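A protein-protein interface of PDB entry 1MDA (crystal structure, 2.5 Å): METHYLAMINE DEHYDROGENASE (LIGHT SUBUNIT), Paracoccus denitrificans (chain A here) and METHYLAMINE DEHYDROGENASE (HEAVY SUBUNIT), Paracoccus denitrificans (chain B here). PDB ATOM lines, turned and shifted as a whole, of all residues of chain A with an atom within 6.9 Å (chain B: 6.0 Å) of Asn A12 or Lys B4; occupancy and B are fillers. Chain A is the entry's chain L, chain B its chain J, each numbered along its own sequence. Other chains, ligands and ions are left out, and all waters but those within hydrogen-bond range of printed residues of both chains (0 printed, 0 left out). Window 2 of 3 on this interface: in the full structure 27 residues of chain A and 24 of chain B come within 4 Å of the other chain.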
ATOM      1  N   GLN A  10       4.489 -30.252   8.973  1.00  0.00           N
ATOM      2  CA  GLN A  10       4.761 -31.263   9.994  1.00  0.00           C
ATOM      3  C   GLN A  10       4.901 -30.604  11.350  1.00  0.00           C
ATOM      4  O   GLN A  10       5.021 -29.376  11.456  1.00  0.00           O
ATOM      5  CB  GLN A  10       5.875 -32.303   9.725  1.00  0.00           C
ATOM      6  CG  GLN A  10       7.287 -31.785   9.373  1.00  0.00           C
ATOM      7  CD  GLN A  10       8.091 -31.179  10.497  1.00  0.00           C
ATOM      8  OE1 GLN A  10       7.650 -31.121  11.651  1.00  0.00           O
ATOM      9  NE2 GLN A  10       9.296 -30.745  10.148  1.00  0.00           N
ATOM     10  N   ASP A  11       4.895 -31.419  12.386  1.00  0.00           N
ATOM     11  CA  ASP A  11       4.940 -30.887  13.743  1.00  0.00           C
ATOM     12  C   ASP A  11       5.891 -31.682  14.605  1.00  0.00           C
ATOM     13  O   ASP A  11       5.564 -32.051  15.714  1.00  0.00           O
ATOM     14  CB  ASP A  11       3.554 -30.921  14.401  1.00  0.00           C
ATOM     15  CG  ASP A  11       3.504 -30.182  15.703  1.00  0.00           C
ATOM     16  OD1 ASP A  11       4.245 -29.262  15.986  1.00  0.00           O
ATOM     17  OD2 ASP A  11       2.657 -30.696  16.546  1.00  0.00           O
ATOM     18  N   ASN A  12       7.086 -31.971  14.086  1.00  0.00           N
ATOM     19  CA  ASN A  12       7.965 -32.756  14.888  1.00  0.00           C
ATOM     20  C   ASN A  12       9.410 -32.359  14.764  1.00  0.00           C
ATOM     21  O   ASN A  12      10.230 -32.847  15.533  1.00  0.00           O
ATOM     22  CB  ASN A  12       7.718 -34.279  14.767  1.00  0.00           C
ATOM     23  CG  ASN A  12       8.032 -34.873  13.408  1.00  0.00           C
ATOM     24  OD1 ASN A  12       9.138 -34.695  12.901  1.00  0.00           O
ATOM     25  ND2 ASN A  12       7.025 -35.484  12.781  1.00  0.00           N
ATOM     26  N   ASP A  13       9.756 -31.502  13.812  1.00  0.00           N
ATOM     27  CA  ASP A  13      11.183 -31.198  13.755  1.00  0.00           C
ATOM     28  C   ASP A  13      11.585 -29.887  14.389  1.00  0.00           C
ATOM     29  O   ASP A  13      12.171 -29.906  15.464  1.00  0.00           O
ATOM     30  CB  ASP A  13      11.900 -31.442  12.428  1.00  0.00           C
ATOM     31  CG  ASP A  13      13.365 -31.704  12.638  1.00  0.00           C
ATOM     32  OD1 ASP A  13      13.986 -30.817  13.369  1.00  0.00           O
ATOM     33  OD2 ASP A  13      13.910 -32.679  12.188  1.00  0.00           O
ATOM     34  N   ILE A  14      11.195 -28.804  13.719  1.00  0.00           N
ATOM     35  CA  ILE A  14      11.450 -27.392  14.013  1.00  0.00           C
ATOM     36  C   ILE A  14      12.709 -26.806  13.428  1.00  0.00           C
ATOM     37  O   ILE A  14      12.798 -25.602  13.194  1.00  0.00           O
ATOM     38  CB  ILE A  14      11.293 -26.883  15.416  1.00  0.00           C
ATOM     39  CG1 ILE A  14      12.443 -27.345  16.292  1.00  0.00           C
ATOM     40  CG2 ILE A  14       9.898 -27.280  15.895  1.00  0.00           C
ATOM     41  CD1 ILE A  14      12.755 -26.399  17.441  1.00  0.00           C
ATOM     42  N   GLN A  15      13.682 -27.655  13.220  1.00  0.00           N
ATOM     43  CA  GLN A  15      14.898 -27.242  12.576  1.00  0.00           C
ATOM     44  C   GLN A  15      14.797 -27.380  11.065  1.00  0.00           C
ATOM     45  O   GLN A  15      15.642 -26.902  10.295  1.00  0.00           O
ATOM     46  CB  GLN A  15      16.194 -27.810  13.225  1.00  0.00           C
ATOM     47  CG  GLN A  15      16.520 -27.069  14.540  1.00  0.00           C
ATOM     48  CD  GLN A  15      17.807 -27.491  15.198  1.00  0.00           C
ATOM     49  OE1 GLN A  15      18.539 -28.316  14.649  1.00  0.00           O
ATOM     50  NE2 GLN A  15      18.047 -26.998  16.414  1.00  0.00           N
ATOM     51  N   TYR A  19       8.425 -27.537   8.701  1.00  0.00           N
ATOM     52  CA  TYR A  19       7.818 -27.328   9.999  1.00  0.00           C
ATOM     53  C   TYR A  19       6.625 -26.371   9.942  1.00  0.00           C
ATOM     54  O   TYR A  19       6.704 -25.252   9.417  1.00  0.00           O
ATOM     55  CB  TYR A  19       8.861 -26.892  11.041  1.00  0.00           C
ATOM     56  CG  TYR A  19       8.222 -26.690  12.381  1.00  0.00           C
ATOM     57  CD1 TYR A  19       7.706 -27.791  13.060  1.00  0.00           C
ATOM     58  CD2 TYR A  19       8.122 -25.433  12.976  1.00  0.00           C
ATOM     59  CE1 TYR A  19       7.063 -27.655  14.281  1.00  0.00           C
ATOM     60  CE2 TYR A  19       7.512 -25.275  14.220  1.00  0.00           C
ATOM     61  CZ  TYR A  19       6.992 -26.397  14.873  1.00  0.00           C
ATOM     62  OH  TYR A  19       6.375 -26.266  16.088  1.00  0.00           O
ATOM     63  N   TRP A  20       5.523 -26.797  10.532  1.00  0.00           N
ATOM     64  CA  TRP A  20       4.278 -26.033  10.535  1.00  0.00           C
ATOM     65  C   TRP A  20       4.365 -24.520  10.725  1.00  0.00           C
ATOM     66  O   TRP A  20       3.834 -23.764   9.924  1.00  0.00           O
ATOM     67  CB  TRP A  20       3.182 -26.689  11.417  1.00  0.00           C
ATOM     68  CG  TRP A  20       2.321 -25.680  12.087  1.00  0.00           C
ATOM     69  CD1 TRP A  20       1.534 -24.750  11.488  1.00  0.00           C
ATOM     70  CD2 TRP A  20       2.319 -25.374  13.476  1.00  0.00           C
ATOM     71  NE1 TRP A  20       1.009 -23.897  12.418  1.00  0.00           N
ATOM     72  CE2 TRP A  20       1.448 -24.270  13.650  1.00  0.00           C
ATOM     73  CE3 TRP A  20       2.905 -25.970  14.580  1.00  0.00           C
ATOM     74  CZ2 TRP A  20       1.124 -23.776  14.902  1.00  0.00           C
ATOM     75  CZ3 TRP A  20       2.619 -25.435  15.821  1.00  0.00           C
ATOM     76  CH2 TRP A  20       1.759 -24.344  15.967  1.00  0.00           C
ATOM     77  N   ASP A  31      16.838 -21.354  16.020  1.00  0.00           N
ATOM     78  CA  ASP A  31      17.208 -22.429  16.899  1.00  0.00           C
ATOM     79  C   ASP A  31      18.559 -23.017  16.496  1.00  0.00           C
ATOM     80  O   ASP A  31      19.294 -23.625  17.285  1.00  0.00           O
ATOM     81  CB  ASP A  31      16.072 -23.447  16.805  1.00  0.00           C
ATOM     82  CG  ASP A  31      15.978 -24.384  17.948  1.00  0.00           C
ATOM     83  OD1 ASP A  31      16.139 -24.050  19.101  1.00  0.00           O
ATOM     84  OD2 ASP A  31      15.776 -25.595  17.539  1.00  0.00           O
ATOM     85  N   GLU B   1      15.995 -34.673  13.323  1.00  0.00           N
ATOM     86  CA  GLU B   1      17.192 -34.642  14.153  1.00  0.00           C
ATOM     87  C   GLU B   1      16.783 -34.224  15.605  1.00  0.00           C
ATOM     88  O   GLU B   1      15.968 -33.339  15.789  1.00  0.00           O
ATOM     89  CB  GLU B   1      18.255 -33.731  13.479  1.00  0.00           C
ATOM     90  CG  GLU B   1      18.000 -33.469  11.963  1.00  0.00           C
ATOM     91  CD  GLU B   1      17.341 -32.129  11.690  1.00  0.00           C
ATOM     92  OE1 GLU B   1      17.752 -31.086  12.155  1.00  0.00           O
ATOM     93  OE2 GLU B   1      16.261 -32.203  10.963  1.00  0.00           O
ATOM     94  N   LYS B   2      17.325 -34.855  16.652  1.00  0.00           N
ATOM     95  CA  LYS B   2      16.923 -34.566  18.030  1.00  0.00           C
ATOM     96  C   LYS B   2      17.180 -33.145  18.532  1.00  0.00           C
ATOM     97  O   LYS B   2      18.089 -32.854  19.318  1.00  0.00           O
ATOM     98  CB  LYS B   2      17.461 -35.605  19.005  1.00  0.00           C
ATOM     99  CG  LYS B   2      16.816 -35.549  20.387  1.00  0.00           C
ATOM    100  CD  LYS B   2      15.346 -35.971  20.382  1.00  0.00           C
ATOM    101  CE  LYS B   2      14.779 -36.175  21.788  1.00  0.00           C
ATOM    102  NZ  LYS B   2      13.426 -36.760  21.829  1.00  0.00           N
ATOM    103  N   SER B   3      16.219 -32.333  18.159  1.00  0.00           N
ATOM    104  CA  SER B   3      16.014 -30.905  18.325  1.00  0.00           C
ATOM    105  C   SER B   3      14.861 -30.809  17.349  1.00  0.00           C
ATOM    106  O   SER B   3      14.757 -30.057  16.387  1.00  0.00           O
ATOM    107  CB  SER B   3      17.259 -30.050  18.085  1.00  0.00           C
ATOM    108  OG  SER B   3      18.247 -30.318  19.092  1.00  0.00           O
ATOM    109  N   LYS B   4      14.127 -31.869  17.661  1.00  0.00           N
ATOM    110  CA  LYS B   4      12.966 -32.519  17.130  1.00  0.00           C
ATOM    111  C   LYS B   4      12.101 -32.553  18.366  1.00  0.00           C
ATOM    112  O   LYS B   4      11.032 -33.148  18.449  1.00  0.00           O
ATOM    113  CB  LYS B   4      13.439 -33.934  16.771  1.00  0.00           C
ATOM    114  CG  LYS B   4      12.637 -34.631  15.695  1.00  0.00           C
ATOM    115  CD  LYS B   4      13.445 -35.697  14.959  1.00  0.00           C
ATOM    116  CE  LYS B   4      13.549 -37.015  15.711  1.00  0.00           C
ATOM    117  NZ  LYS B   4      14.086 -36.875  17.071  1.00  0.00           N
ATOM    118  N   VAL B   5      12.745 -31.960  19.373  1.00  0.00           N
ATOM    119  CA  VAL B   5      12.198 -31.614  20.658  1.00  0.00           C
ATOM    120  C   VAL B   5      11.819 -30.138  20.565  1.00  0.00           C
ATOM    121  O   VAL B   5      12.505 -29.157  20.867  1.00  0.00           O
ATOM    122  CB  VAL B   5      13.073 -32.000  21.827  1.00  0.00           C
ATOM    123  CG1 VAL B   5      14.522 -31.634  21.525  1.00  0.00           C
ATOM    124  CG2 VAL B   5      12.567 -31.267  23.069  1.00  0.00           C
ATOM    125  N   ALA B   6      10.674 -30.072  19.984  1.00  0.00           N
ATOM    126  CA  ALA B   6       9.918 -28.946  19.589  1.00  0.00           C
ATOM    127  C   ALA B   6       8.673 -29.701  19.223  1.00  0.00           C
ATOM    128  O   ALA B   6       8.280 -29.962  18.076  1.00  0.00           O
ATOM    129  CB  ALA B   6      10.624 -28.216  18.486  1.00  0.00           C
ATOM    130  N   GLY B   7       8.441 -30.320  20.374  1.00  0.00           N
ATOM    131  CA  GLY B   7       7.447 -31.187  20.923  1.00  0.00           C
ATOM    132  C   GLY B   7       7.339 -30.591  22.323  1.00  0.00           C
ATOM    133  O   GLY B   7       6.500 -30.949  23.157  1.00  0.00           O
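OD1 of Asp A13 is in hydrogen-bond range of N of Gln A15, at 3.2 Å.
The side-chain amide oxygen of Gln A10 lies within hydrogen-bond range of the backbone NH of Asp A13.
The side-chain amide nitrogen of Gln A15 is in hydrogen-bond range of the side-chain carboxylate of Asp A31 (2.9 Å).
The backbone NH of Asn A12 lies within hydrogen-bond range of the side-chain amide oxygen of Gln A10, at 2.6 Å.
O of Asp A13 touches CA of Lys B4, 3.2 Å away.
CB of Ala B6 touches O of Asp A13, at 3.8 Å.
Ile A14 touches Ser B3 (CG1 to O, 3.6 Å).
Ala B6 touches Ile A14.
Glu B1 touches Gln A15 (OE1 to CB, 3.8 Å).
Gln A15 touches Ser B3 (NE2 to CB, 3.6 Å).
Of chain B, only Lys B4 (3.0 Å) comes within 4 Å of Asn A12.
Lys B4 touches just these residues of chain A: Asn A12 (3.0 Å) and Asp A13 (3.2 Å).
Of the printed residues of chain A, Ala B6 touches Asp A13 (3.8 Å) and Ile A14 (2.8 Å).
Printed residues of chain B within 4 Å of Ile A14: Ser B3 and Ala B6.
Of the printed residues of chain A, Glu B1 touches Asp A13 and Gln A15.
Asp A31 touches none of the printed residues of chain B.
Tyr A19 touches none of the printed residues of chain B.
The nearest residue of chain A that does not touch Lys B4 is Ile A14 (5.0 Å).
The nearest printed residue of chain B that does not touch Ile A14 is Val B5 (4.4 Å).
Of the 9 printed residues of chain A, 4 touch a printed residue of chain B.
Hydrophobic or aromatic side chains of chain B within 4 Å of the printed part of chain A: Ala B6.
Among the printed residues, 9 pairs touch across the chains.
N of Glu B1 is in hydrogen-bond range of OD2 of Asp A13.
O of Asp A13 lies close to O of Ser B3 (2.7 Å).
The backbone carbonyl oxygen (O) of Lys B4 lies close to the backbone carbonyl oxygen (O) of Asn A12.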
